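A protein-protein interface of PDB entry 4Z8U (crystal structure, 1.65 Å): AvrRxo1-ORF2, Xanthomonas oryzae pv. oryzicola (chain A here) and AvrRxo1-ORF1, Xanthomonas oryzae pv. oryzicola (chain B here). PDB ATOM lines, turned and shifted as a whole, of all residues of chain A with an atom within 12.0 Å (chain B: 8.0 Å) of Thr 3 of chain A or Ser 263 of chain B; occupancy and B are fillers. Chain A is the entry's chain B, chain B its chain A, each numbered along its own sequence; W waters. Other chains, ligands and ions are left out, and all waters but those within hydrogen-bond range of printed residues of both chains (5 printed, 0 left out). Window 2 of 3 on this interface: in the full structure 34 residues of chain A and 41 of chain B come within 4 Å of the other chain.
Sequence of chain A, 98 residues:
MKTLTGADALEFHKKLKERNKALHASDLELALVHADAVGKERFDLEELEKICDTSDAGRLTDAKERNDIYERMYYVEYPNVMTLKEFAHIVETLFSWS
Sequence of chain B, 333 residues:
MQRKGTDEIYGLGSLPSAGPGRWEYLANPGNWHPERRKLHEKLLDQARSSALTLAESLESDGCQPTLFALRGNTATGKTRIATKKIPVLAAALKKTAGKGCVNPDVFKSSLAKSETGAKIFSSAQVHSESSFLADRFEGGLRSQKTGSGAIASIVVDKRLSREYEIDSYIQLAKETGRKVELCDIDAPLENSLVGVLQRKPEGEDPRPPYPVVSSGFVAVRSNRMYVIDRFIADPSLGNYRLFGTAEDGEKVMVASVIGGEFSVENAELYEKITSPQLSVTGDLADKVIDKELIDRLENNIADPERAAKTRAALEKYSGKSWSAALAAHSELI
SD of Met 1 of chain A sits at hydrogen-bond distance from N of Ala 267 of chain B.
A ring nitrogen (ND1) of His 13 of chain A is in hydrogen-bond range of the side-chain hydroxyl (OH) of Tyr 270 of chain B.
The side-chain sulfur of Met 1 of chain A lies close to the side-chain amide oxygen of Asn 266 of chain B (3.8 Å).
N of Val 264 of chain B lies within hydrogen-bond range of O of Leu 4 of chain A (2.9 Å).
The backbone carbonyl oxygen of Ser 263 of chain B lies within hydrogen-bond range of the backbone NH of Ser 256 of chain B, at 3.0 Å.
The side-chain hydroxyl (OG) of Ser 256 of chain B sits at hydrogen-bond distance from the side-chain carboxylate (OE1) of Glu 265 of chain B.
O of Val 254 of chain B lies within hydrogen-bond range of N of Asn 266 of chain B, at 3.0 Å.
N of Ala 255 of chain B sits close to OE2 of Glu 265 of chain B.
The backbone carbonyl oxygen (O) of Val 254 of chain B sits at hydrogen-bond distance from the backbone NH (N) of Glu 265 of chain B, 2.9 Å away.
Among the printed residues, pairs that only touch across the chains: Met 1 of chain A with Glu 265 of chain B (3.8 Å), Thr 3 of chain A with Ser 263 of chain B (3.9 Å), Thr 3 of chain A with Val 264 of chain B (3.6 Å), Thr 3 of chain A with Glu 265 of chain B (3.7 Å), Leu 4 of chain A with Ser 263 of chain B (3.4 Å), Leu 4 of chain A with Ala 267 of chain B (3.9 Å), Ala 9 of chain A with Phe 262 of chain B (3.3 Å), Phe 12 of chain A with Ala 267 of chain B (3.6 Å), His 13 of chain A with Ile 228 of chain B (3.7 Å), His 13 of chain A with Ile 232 of chain B (3.7 Å), His 13 of chain A with Phe 262 of chain B (3.5 Å) and Leu 16 of chain A with Tyr 270 of chain B (3.6 Å).
Thr 3 of chain A touches just these residues of chain B: Ser 263, Val 264 and Glu 265.
Ser 263 of chain B touches two residues of chain A.
Ser 256 of chain B touches none of the printed residues of chain A.
No residue of chain A comes within 4 Å of Glu 261 of chain B.
Of chain A, only Thr 3 and Leu 4 come within 4 Å of Val 264 of chain B.
Printed residues of chain A within 4 Å of Glu 265 of chain B: Met 1 (3.8 Å) and Thr 3 (3.7 Å).
Of the printed residues of chain B, Ala 9 of chain A touches Phe 262 (3.3 Å).
Of the printed residues of chain A, Ala 267 of chain B touches Met 1 (3.8 Å), Leu 4 (3.9 Å) and Phe 12 (3.6 Å).
Tyr 240 of chain B touches none of the printed residues of chain A.
Thr 5 of chain A touches none of the printed residues of chain B.
The nearest printed residue of chain A that does not touch Asn 266 of chain B is Lys 2 of chain A (5.7 Å).
Hydrophobic or aromatic side chains of chain B within 4 Å of the printed part of chain A: Ile 228, Ile 232, Phe 262, Ala 267 and Tyr 270.
Hydrophobic or aromatic side chains of chain A within 4 Å of the printed part of chain B: Met 1, Leu 4, Ala 9, Phe 12, His 13 and Leu 16.
Among the printed residues, 16 pairs touch across the chains.
Water W2 lies within hydrogen-bond range of O of Met 1 of chain A, OG1 of Thr 3 of chain A and O of Glu 265 of chain B.
Water W4 lies within hydrogen-bond range of N of Met 1 of chain A, O of Glu 265 of chain B and ND2 of Asn 266 of chain B.
Water W3 lies within hydrogen-bond range of the backbone carbonyl oxygen of Phe 262 of chain B, the backbone NH of Gly 6 of chain A, the side-chain hydroxyl of Ser 263 of chain B and the side-chain carboxylate of Glu 261 of chain B.
Water W1 lies within hydrogen-bond range of the backbone carbonyl oxygen of Lys 2 of chain A (2.8 Å), the backbone NH of Ala 267 of chain B (2.9 Å) and the backbone carbonyl oxygen of Val 264 of chain B (3.0 Å).
Water W5 lies within hydrogen-bond range of the backbone carbonyl oxygen (O) of Gly 6 of chain A (2.8 Å) and the backbone carbonyl oxygen (O) of Phe 262 of chain B (2.8 Å).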
ATOM      1  N   MET A   1     -17.637  -9.363 -14.577  1.00  0.00           N
ATOM      2  CA  MET A   1     -16.399  -8.783 -13.983  1.00  0.00           C
ATOM      3  C   MET A   1     -16.677  -8.308 -12.536  1.00  0.00           C
ATOM      4  O   MET A   1     -17.805  -8.079 -12.149  1.00  0.00           O
ATOM      5  CB  MET A   1     -15.845  -7.707 -14.962  1.00  0.00           C
ATOM      6  CG  MET A   1     -16.679  -6.390 -15.122  1.00  0.00           C
ATOM      7  SD  MET A   1     -15.724  -5.314 -16.468  1.00  0.00           S
ATOM      8  CE  MET A   1     -14.355  -4.601 -15.323  1.00  0.00           C
ATOM      9  N   LYS A   2     -15.597  -8.161 -11.763  1.00  0.00           N
ATOM     10  CA  LYS A   2     -15.631  -7.636 -10.439  1.00  0.00           C
ATOM     11  C   LYS A   2     -16.311  -6.226 -10.390  1.00  0.00           C
ATOM     12  O   LYS A   2     -15.960  -5.341 -11.218  1.00  0.00           O
ATOM     13  CB  LYS A   2     -14.176  -7.571  -9.938  1.00  0.00           C
ATOM     14  CG  LYS A   2     -13.106  -7.294 -11.048  1.00  0.00           C
ATOM     15  CD  LYS A   2     -12.401  -8.547 -11.665  1.00  0.00           C
ATOM     16  CE  LYS A   2     -12.825  -8.957 -13.101  1.00  0.00           C
ATOM     17  NZ  LYS A   2     -12.244  -8.070 -14.166  1.00  0.00           N
ATOM     18  N   THR A   3     -17.243  -6.051  -9.440  1.00  0.00           N
ATOM     19  CA  THR A   3     -17.896  -4.723  -9.217  1.00  0.00           C
ATOM     20  C   THR A   3     -16.960  -3.708  -8.620  1.00  0.00           C
ATOM     21  O   THR A   3     -16.325  -3.990  -7.654  1.00  0.00           O
ATOM     22  CB  THR A   3     -19.194  -4.832  -8.290  1.00  0.00           C
ATOM     23  OG1 THR A   3     -20.114  -5.695  -8.964  1.00  0.00           O
ATOM     24  CG2 THR A   3     -19.816  -3.539  -8.114  1.00  0.00           C
ATOM     25  N   LEU A   4     -16.874  -2.541  -9.232  1.00  0.00           N
ATOM     26  CA  LEU A   4     -16.182  -1.422  -8.589  1.00  0.00           C
ATOM     27  C   LEU A   4     -17.079  -0.813  -7.515  1.00  0.00           C
ATOM     28  O   LEU A   4     -18.227  -0.429  -7.769  1.00  0.00           O
ATOM     29  CB  LEU A   4     -15.777  -0.330  -9.578  1.00  0.00           C
ATOM     30  CG  LEU A   4     -15.080  -0.753 -10.864  1.00  0.00           C
ATOM     31  CD1 LEU A   4     -14.749   0.485 -11.686  1.00  0.00           C
ATOM     32  CD2 LEU A   4     -13.874  -1.617 -10.573  1.00  0.00           C
ATOM     33  N   THR A   5     -16.500  -0.558  -6.340  1.00  0.00           N
ATOM     34  CA  THR A   5     -17.299  -0.122  -5.225  1.00  0.00           C
ATOM     35  C   THR A   5     -16.584   1.071  -4.555  1.00  0.00           C
ATOM     36  O   THR A   5     -15.397   1.328  -4.860  1.00  0.00           O
ATOM     37  CB  THR A   5     -17.441  -1.193  -4.116  1.00  0.00           C
ATOM     38  OG1 THR A   5     -16.137  -1.392  -3.550  1.00  0.00           O
ATOM     39  CG2 THR A   5     -17.886  -2.524  -4.726  1.00  0.00           C
ATOM     40  N   GLY A   6     -17.292   1.789  -3.694  1.00  0.00           N
ATOM     41  CA  GLY A   6     -16.707   2.836  -2.933  1.00  0.00           C
ATOM     42  C   GLY A   6     -15.862   3.808  -3.709  1.00  0.00           C
ATOM     43  O   GLY A   6     -16.314   4.415  -4.695  1.00  0.00           O
ATOM     44  N   ALA A   7     -14.643   4.044  -3.213  1.00  0.00           N
ATOM     45  CA  ALA A   7     -13.832   5.124  -3.854  1.00  0.00           C
ATOM     46  C   ALA A   7     -13.425   4.721  -5.275  1.00  0.00           C
ATOM     47  O   ALA A   7     -13.271   5.615  -6.117  1.00  0.00           O
ATOM     48  CB  ALA A   7     -12.577   5.449  -2.990  1.00  0.00           C
ATOM     49  N   ASP A   8     -13.205   3.442  -5.523  1.00  0.00           N
ATOM     50  CA  ASP A   8     -12.821   3.024  -6.925  1.00  0.00           C
ATOM     51  C   ASP A   8     -13.973   3.343  -7.866  1.00  0.00           C
ATOM     52  O   ASP A   8     -13.757   3.821  -9.009  1.00  0.00           O
ATOM     53  CB  ASP A   8     -12.531   1.548  -6.981  1.00  0.00           C
ATOM     54  CG  ASP A   8     -11.188   1.184  -6.345  1.00  0.00           C
ATOM     55  OD1 ASP A   8     -10.312   2.066  -6.178  1.00  0.00           O
ATOM     56  OD2 ASP A   8     -11.044   0.002  -6.019  1.00  0.00           O
ATOM     57  N   ALA A   9     -15.194   3.110  -7.424  1.00  0.00           N
ATOM     58  CA  ALA A   9     -16.317   3.426  -8.314  1.00  0.00           C
ATOM     59  C   ALA A   9     -16.414   4.904  -8.584  1.00  0.00           C
ATOM     60  O   ALA A   9     -16.597   5.346  -9.730  1.00  0.00           O
ATOM     61  CB  ALA A   9     -17.664   2.885  -7.751  1.00  0.00           C
ATOM     62  N   LEU A  10     -16.254   5.713  -7.502  1.00  0.00           N
ATOM     63  CA  LEU A  10     -16.369   7.107  -7.685  1.00  0.00           C
ATOM     64  C   LEU A  10     -15.236   7.657  -8.613  1.00  0.00           C
ATOM     65  O   LEU A  10     -15.482   8.524  -9.439  1.00  0.00           O
ATOM     66  CB  LEU A  10     -16.286   7.849  -6.354  1.00  0.00           C
ATOM     67  CG  LEU A  10     -17.611   7.890  -5.557  1.00  0.00           C
ATOM     68  CD1 LEU A  10     -17.325   8.462  -4.147  1.00  0.00           C
ATOM     69  CD2 LEU A  10     -18.637   8.787  -6.248  1.00  0.00           C
ATOM     70  N   GLU A  11     -14.031   7.163  -8.361  1.00  0.00           N
ATOM     71  CA  GLU A  11     -12.870   7.628  -9.244  1.00  0.00           C
ATOM     72  C   GLU A  11     -13.042   7.164 -10.707  1.00  0.00           C
ATOM     73  O   GLU A  11     -12.821   7.961 -11.596  1.00  0.00           O
ATOM     74  CB  GLU A  11     -11.560   7.178  -8.669  1.00  0.00           C
ATOM     75  CG  GLU A  11     -10.347   7.775  -9.395  1.00  0.00           C
ATOM     76  CD  GLU A  11     -10.165   9.266  -9.145  1.00  0.00           C
ATOM     77  OE1 GLU A  11     -10.951   9.868  -8.378  1.00  0.00           O
ATOM     78  OE2 GLU A  11      -9.205   9.859  -9.725  1.00  0.00           O
ATOM     79  N   PHE A  12     -13.522   5.944 -10.932  1.00  0.00           N
ATOM     80  CA  PHE A  12     -13.835   5.529 -12.317  1.00  0.00           C
ATOM     81  C   PHE A  12     -14.845   6.502 -12.954  1.00  0.00           C
ATOM     82  O   PHE A  12     -14.685   6.964 -14.087  1.00  0.00           O
ATOM     83  CB  PHE A  12     -14.369   4.082 -12.336  1.00  0.00           C
ATOM     84  CG  PHE A  12     -14.336   3.414 -13.707  1.00  0.00           C
ATOM     85  CD1 PHE A  12     -13.217   2.732 -14.131  1.00  0.00           C
ATOM     86  CD2 PHE A  12     -15.386   3.561 -14.579  1.00  0.00           C
ATOM     87  CE1 PHE A  12     -13.145   2.124 -15.379  1.00  0.00           C
ATOM     88  CE2 PHE A  12     -15.339   2.904 -15.848  1.00  0.00           C
ATOM     89  CZ  PHE A  12     -14.222   2.159 -16.204  1.00  0.00           C
ATOM     90  N   HIS A  13     -15.933   6.800 -12.239  1.00  0.00           N
ATOM     91  CA  HIS A  13     -16.980   7.661 -12.769  1.00  0.00           C
ATOM     92  C   HIS A  13     -16.426   9.059 -13.052  1.00  0.00           C
ATOM     93  O   HIS A  13     -16.641   9.638 -14.093  1.00  0.00           O
ATOM     94  CB  HIS A  13     -18.114   7.663 -11.699  1.00  0.00           C
ATOM     95  CG  HIS A  13     -19.245   8.599 -12.008  1.00  0.00           C
ATOM     96  ND1 HIS A  13     -20.313   8.219 -12.809  1.00  0.00           N
ATOM     97  CD2 HIS A  13     -19.482   9.898 -11.645  1.00  0.00           C
ATOM     98  CE1 HIS A  13     -21.190   9.216 -12.864  1.00  0.00           C
ATOM     99  NE2 HIS A  13     -20.666  10.286 -12.163  1.00  0.00           N
ATOM    100  N   LYS A  14     -15.562   9.566 -12.136  1.00  0.00           N
ATOM    101  CA  LYS A  14     -15.013  10.926 -12.314  1.00  0.00           C
ATOM    102  C   LYS A  14     -14.081  10.981 -13.590  1.00  0.00           C
ATOM    103  O   LYS A  14     -14.218  11.899 -14.428  1.00  0.00           O
ATOM    104  CB  LYS A  14     -14.054  11.250 -11.102  1.00  0.00           C
ATOM    105  CG  LYS A  14     -13.567  12.674 -11.218  1.00  0.00           C
ATOM    106  CD  LYS A  14     -12.795  12.961  -9.893  1.00  0.00           C
ATOM    107  CE  LYS A  14     -12.386  14.416  -9.873  1.00  0.00           C
ATOM    108  NZ  LYS A  14     -11.542  14.579  -8.611  1.00  0.00           N
ATOM    109  N   LEU A  16     -14.125   8.869 -16.159  1.00  0.00           N
ATOM    110  CA  LEU A  16     -14.937   8.620 -17.326  1.00  0.00           C
ATOM    111  C   LEU A  16     -15.678   9.894 -17.761  1.00  0.00           C
ATOM    112  O   LEU A  16     -15.849  10.180 -18.946  1.00  0.00           O
ATOM    113  CB  LEU A  16     -15.924   7.448 -17.050  1.00  0.00           C
ATOM    114  CG  LEU A  16     -16.804   7.050 -18.224  1.00  0.00           C
ATOM    115  CD1 LEU A  16     -16.049   6.666 -19.511  1.00  0.00           C
ATOM    116  CD2 LEU A  16     -17.648   5.873 -17.729  1.00  0.00           C
ATOM    117  N   ILE B 228     -27.043  10.102 -13.652  1.00  0.00           N
ATOM    118  CA  ILE B 228     -26.434   9.350 -12.567  1.00  0.00           C
ATOM    119  C   ILE B 228     -25.924  10.329 -11.473  1.00  0.00           C
ATOM    120  O   ILE B 228     -26.145  10.042 -10.278  1.00  0.00           O
ATOM    121  CB  ILE B 228     -25.277   8.506 -13.142  1.00  0.00           C
ATOM    122  CG1 ILE B 228     -25.916   7.422 -14.056  1.00  0.00           C
ATOM    123  CG2 ILE B 228     -24.509   7.861 -11.984  1.00  0.00           C
ATOM    124  CD1 ILE B 228     -24.898   6.509 -14.805  1.00  0.00           C
ATOM    125  N   ILE B 232     -26.220  10.412  -7.397  1.00  0.00           N
ATOM    126  CA  ILE B 232     -24.997  10.366  -6.576  1.00  0.00           C
ATOM    127  C   ILE B 232     -25.081  11.548  -5.624  1.00  0.00           C
ATOM    128  O   ILE B 232     -24.702  11.424  -4.433  1.00  0.00           O
ATOM    129  CB  ILE B 232     -23.732  10.415  -7.446  1.00  0.00           C
ATOM    130  CG1 ILE B 232     -23.537   9.031  -8.166  1.00  0.00           C
ATOM    131  CG2 ILE B 232     -22.492  10.552  -6.533  1.00  0.00           C
ATOM    132  CD1 ILE B 232     -22.280   9.010  -9.109  1.00  0.00           C
ATOM    133  N   TYR B 240     -31.368   4.626  -8.686  1.00  0.00           N
ATOM    134  CA  TYR B 240     -31.045   4.596 -10.135  1.00  0.00           C
ATOM    135  C   TYR B 240     -30.366   3.229 -10.413  1.00  0.00           C
ATOM    136  O   TYR B 240     -29.441   2.790  -9.722  1.00  0.00           O
ATOM    137  CB  TYR B 240     -29.999   5.663 -10.457  1.00  0.00           C
ATOM    138  CG  TYR B 240     -29.451   5.640 -11.851  1.00  0.00           C
ATOM    139  CD1 TYR B 240     -28.370   4.778 -12.163  1.00  0.00           C
ATOM    140  CD2 TYR B 240     -30.104   6.323 -12.875  1.00  0.00           C
ATOM    141  CE1 TYR B 240     -27.873   4.706 -13.436  1.00  0.00           C
ATOM    142  CE2 TYR B 240     -29.601   6.244 -14.197  1.00  0.00           C
ATOM    143  CZ  TYR B 240     -28.497   5.411 -14.454  1.00  0.00           C
ATOM    144  OH  TYR B 240     -28.002   5.331 -15.752  1.00  0.00           O
ATOM    145  N   LEU B 242     -28.797   1.137 -14.063  1.00  0.00           N
ATOM    146  CA  LEU B 242     -28.541   1.206 -15.508  1.00  0.00           C
ATOM    147  C   LEU B 242     -28.305  -0.238 -15.958  1.00  0.00           C
ATOM    148  O   LEU B 242     -27.445  -0.890 -15.403  1.00  0.00           O
ATOM    149  CB  LEU B 242     -27.247   1.880 -15.747  1.00  0.00           C
ATOM    150  CG  LEU B 242     -26.689   1.844 -17.207  1.00  0.00           C
ATOM    151  CD1 LEU B 242     -27.667   2.404 -18.250  1.00  0.00           C
ATOM    152  CD2 LEU B 242     -25.384   2.637 -17.149  1.00  0.00           C
ATOM    153  N   MET B 253     -26.635  -5.639 -15.384  1.00  0.00           N
ATOM    154  CA  MET B 253     -26.514  -4.435 -14.572  1.00  0.00           C
ATOM    155  C   MET B 253     -25.157  -3.812 -14.861  1.00  0.00           C
ATOM    156  O   MET B 253     -24.167  -4.526 -15.018  1.00  0.00           O
ATOM    157  CB  MET B 253     -26.640  -4.770 -13.087  1.00  0.00           C
ATOM    158  CG  MET B 253     -26.596  -3.557 -12.171  1.00  0.00           C
ATOM    159  SD  MET B 253     -27.963  -2.507 -11.849  1.00  0.00           S
ATOM    160  CE  MET B 253     -28.901  -3.690 -10.615  1.00  0.00           C
ATOM    161  N   VAL B 254     -25.112  -2.476 -14.986  1.00  0.00           N
ATOM    162  CA  VAL B 254     -23.856  -1.860 -15.434  1.00  0.00           C
ATOM    163  C   VAL B 254     -23.389  -0.850 -14.354  1.00  0.00           C
ATOM    164  O   VAL B 254     -22.248  -0.864 -14.009  1.00  0.00           O
ATOM    165  CB  VAL B 254     -24.070  -1.124 -16.767  1.00  0.00           C
ATOM    166  CG1 VAL B 254     -22.778  -0.313 -17.129  1.00  0.00           C
ATOM    167  CG2 VAL B 254     -24.241  -2.225 -17.907  1.00  0.00           C
ATOM    168  N   ALA B 255     -24.349  -0.078 -13.837  1.00  0.00           N
ATOM    169  CA  ALA B 255     -24.004   0.866 -12.718  1.00  0.00           C
ATOM    170  C   ALA B 255     -25.294   1.099 -11.930  1.00  0.00           C
ATOM    171  O   ALA B 255     -26.383   0.944 -12.457  1.00  0.00           O
ATOM    172  CB  ALA B 255     -23.491   2.226 -13.296  1.00  0.00           C
ATOM    173  N   SER B 256     -25.144   1.542 -10.693  1.00  0.00           N
ATOM    174  CA  SER B 256     -26.344   1.767  -9.817  1.00  0.00           C
ATOM    175  C   SER B 256     -26.104   2.766  -8.710  1.00  0.00           C
ATOM    176  O   SER B 256     -24.946   2.920  -8.216  1.00  0.00           O
ATOM    177  CB  SER B 256     -26.814   0.398  -9.194  1.00  0.00           C
ATOM    178  OG  SER B 256     -25.762  -0.151  -8.410  1.00  0.00           O
ATOM    179  N   VAL B 257     -27.158   3.468  -8.294  1.00  0.00           N
ATOM    180  CA  VAL B 257     -27.044   4.269  -7.089  1.00  0.00           C
ATOM    181  C   VAL B 257     -28.298   3.831  -6.269  1.00  0.00           C
ATOM    182  O   VAL B 257     -29.422   4.088  -6.662  1.00  0.00           O
ATOM    183  CB  VAL B 257     -27.181   5.746  -7.381  1.00  0.00           C
ATOM    184  CG1 VAL B 257     -26.763   6.540  -6.078  1.00  0.00           C
ATOM    185  CG2 VAL B 257     -26.207   6.138  -8.537  1.00  0.00           C
ATOM    186  N   ILE B 258     -28.034   3.064  -5.234  1.00  0.00           N
ATOM    187  CA  ILE B 258     -29.136   2.487  -4.453  1.00  0.00           C
ATOM    188  C   ILE B 258     -28.876   2.812  -3.001  1.00  0.00           C
ATOM    189  O   ILE B 258     -27.848   2.468  -2.471  1.00  0.00           O
ATOM    190  CB  ILE B 258     -29.146   0.948  -4.683  1.00  0.00           C
ATOM    191  CG1 ILE B 258     -29.461   0.602  -6.155  1.00  0.00           C
ATOM    192  CG2 ILE B 258     -30.261   0.285  -3.743  1.00  0.00           C
ATOM    193  CD1 ILE B 258     -29.179  -0.887  -6.536  1.00  0.00           C
ATOM    194  N   GLY B 260     -28.202   5.482  -1.851  1.00  0.00           N
ATOM    195  CA  GLY B 260     -27.094   6.417  -1.861  1.00  0.00           C
ATOM    196  C   GLY B 260     -25.789   5.774  -2.284  1.00  0.00           C
ATOM    197  O   GLY B 260     -24.772   6.423  -2.386  1.00  0.00           O
ATOM    198  N   GLU B 261     -25.747   4.453  -2.406  1.00  0.00           N
ATOM    199  CA  GLU B 261     -24.508   3.822  -2.644  1.00  0.00           C
ATOM    200  C   GLU B 261     -24.269   3.678  -4.128  1.00  0.00           C
ATOM    201  O   GLU B 261     -25.085   3.049  -4.796  1.00  0.00           O
ATOM    202  CB  GLU B 261     -24.491   2.406  -2.032  1.00  0.00           C
ATOM    203  CG  GLU B 261     -23.125   1.714  -2.039  1.00  0.00           C
ATOM    204  CD  GLU B 261     -22.659   1.172  -0.652  1.00  0.00           C
ATOM    205  OE1 GLU B 261     -23.233   1.549   0.398  1.00  0.00           O
ATOM    206  OE2 GLU B 261     -21.679   0.406  -0.659  1.00  0.00           O
ATOM    207  N   PHE B 262     -23.149   4.183  -4.613  1.00  0.00           N
ATOM    208  CA  PHE B 262     -22.826   4.080  -6.061  1.00  0.00           C
ATOM    209  C   PHE B 262     -21.857   2.928  -6.367  1.00  0.00           C
ATOM    210  O   PHE B 262     -20.815   2.767  -5.678  1.00  0.00           O
ATOM    211  CB  PHE B 262     -22.207   5.400  -6.477  1.00  0.00           C
ATOM    212  CG  PHE B 262     -21.699   5.378  -7.908  1.00  0.00           C
ATOM    213  CD1 PHE B 262     -22.610   5.139  -9.014  1.00  0.00           C
ATOM    214  CD2 PHE B 262     -20.364   5.653  -8.200  1.00  0.00           C
ATOM    215  CE1 PHE B 262     -22.170   5.149 -10.329  1.00  0.00           C
ATOM    216  CE2 PHE B 262     -19.909   5.573  -9.558  1.00  0.00           C
ATOM    217  CZ  PHE B 262     -20.808   5.334 -10.606  1.00  0.00           C
ATOM    218  N   SER B 263     -22.151   2.103  -7.346  1.00  0.00           N
ATOM    219  CA  SER B 263     -21.311   1.021  -7.695  1.00  0.00           C
ATOM    220  C   SER B 263     -21.337   0.836  -9.221  1.00  0.00           C
ATOM    221  O   SER B 263     -22.286   1.259  -9.898  1.00  0.00           O
ATOM    222  CB  SER B 263     -21.902  -0.334  -7.159  1.00  0.00           C
ATOM    223  OG  SER B 263     -22.030  -0.192  -5.779  1.00  0.00           O
ATOM    224  N   VAL B 264     -20.240   0.317  -9.730  1.00  0.00           N
ATOM    225  CA  VAL B 264     -20.158   0.072 -11.183  1.00  0.00           C
ATOM    226  C   VAL B 264     -20.038  -1.434 -11.329  1.00  0.00           C
ATOM    227  O   VAL B 264     -18.944  -1.960 -11.251  1.00  0.00           O
ATOM    228  CB  VAL B 264     -19.005   0.787 -11.844  1.00  0.00           C
ATOM    229  CG1 VAL B 264     -18.999   0.445 -13.377  1.00  0.00           C
ATOM    230  CG2 VAL B 264     -19.215   2.298 -11.610  1.00  0.00           C
ATOM    231  N   GLU B 265     -21.146  -2.105 -11.642  1.00  0.00           N
ATOM    232  CA  GLU B 265     -21.119  -3.548 -11.785  1.00  0.00           C
ATOM    233  C   GLU B 265     -20.468  -4.068 -13.086  1.00  0.00           C
ATOM    234  O   GLU B 265     -20.074  -5.251 -13.164  1.00  0.00           O
ATOM    235  CB  GLU B 265     -22.552  -4.126 -11.670  1.00  0.00           C
ATOM    236  CG  GLU B 265     -23.251  -3.922 -10.271  1.00  0.00           C
ATOM    237  CD  GLU B 265     -23.885  -2.560 -10.101  1.00  0.00           C
ATOM    238  OE1 GLU B 265     -24.537  -2.289  -9.021  1.00  0.00           O
ATOM    239  OE2 GLU B 265     -23.848  -1.726 -11.050  1.00  0.00           O
ATOM    240  N   ASN B 266     -20.366  -3.217 -14.119  1.00  0.00           N
ATOM    241  CA  ASN B 266     -19.655  -3.624 -15.304  1.00  0.00           C
ATOM    242  C   ASN B 266     -18.951  -2.404 -15.917  1.00  0.00           C
ATOM    243  O   ASN B 266     -19.514  -1.650 -16.702  1.00  0.00           O
ATOM    244  CB  ASN B 266     -20.621  -4.257 -16.341  1.00  0.00           C
ATOM    245  CG  ASN B 266     -19.854  -4.950 -17.523  1.00  0.00           C
ATOM    246  OD1 ASN B 266     -18.975  -4.352 -18.162  1.00  0.00           O
ATOM    247  ND2 ASN B 266     -20.184  -6.161 -17.775  1.00  0.00           N
ATOM    248  N   ALA B 267     -17.719  -2.244 -15.517  1.00  0.00           N
ATOM    249  CA  ALA B 267     -16.971  -1.021 -15.913  1.00  0.00           C
ATOM    250  C   ALA B 267     -16.700  -0.938 -17.435  1.00  0.00           C
ATOM    251  O   ALA B 267     -16.677   0.148 -18.002  1.00  0.00           O
ATOM    252  CB  ALA B 267     -15.605  -1.010 -15.183  1.00  0.00           C
ATOM    253  N   TYR B 270     -19.862   0.239 -18.891  1.00  0.00           N
ATOM    254  CA  TYR B 270     -20.109   1.616 -18.423  1.00  0.00           C
ATOM    255  C   TYR B 270     -19.330   2.622 -19.292  1.00  0.00           C
ATOM    256  O   TYR B 270     -19.849   3.730 -19.643  1.00  0.00           O
ATOM    257  CB  TYR B 270     -19.711   1.722 -16.953  1.00  0.00           C
ATOM    258  CG  TYR B 270     -20.188   3.045 -16.286  1.00  0.00           C
ATOM    259  CD1 TYR B 270     -21.458   3.509 -16.419  1.00  0.00           C
ATOM    260  CD2 TYR B 270     -19.335   3.707 -15.361  1.00  0.00           C
ATOM    261  CE1 TYR B 270     -21.940   4.634 -15.774  1.00  0.00           C
ATOM    262  CE2 TYR B 270     -19.790   4.875 -14.703  1.00  0.00           C
ATOM    263  CZ  TYR B 270     -21.061   5.307 -14.829  1.00  0.00           C
ATOM    264  OH  TYR B 270     -21.532   6.426 -14.245  1.00  0.00           O
HETATM  265  O   HOH W   1     -16.965  -3.432 -12.973  1.00  0.00           O
HETATM  266  O   HOH W   2     -20.001  -7.478 -11.098  1.00  0.00           O
HETATM  267  O   HOH W   3     -20.145   0.915  -3.729  1.00  0.00           O
HETATM  268  O   HOH W   4     -19.636  -7.546 -14.788  1.00  0.00           O
HETATM  269  O   HOH W   5     -19.092   4.753  -4.701  1.00  0.00           O
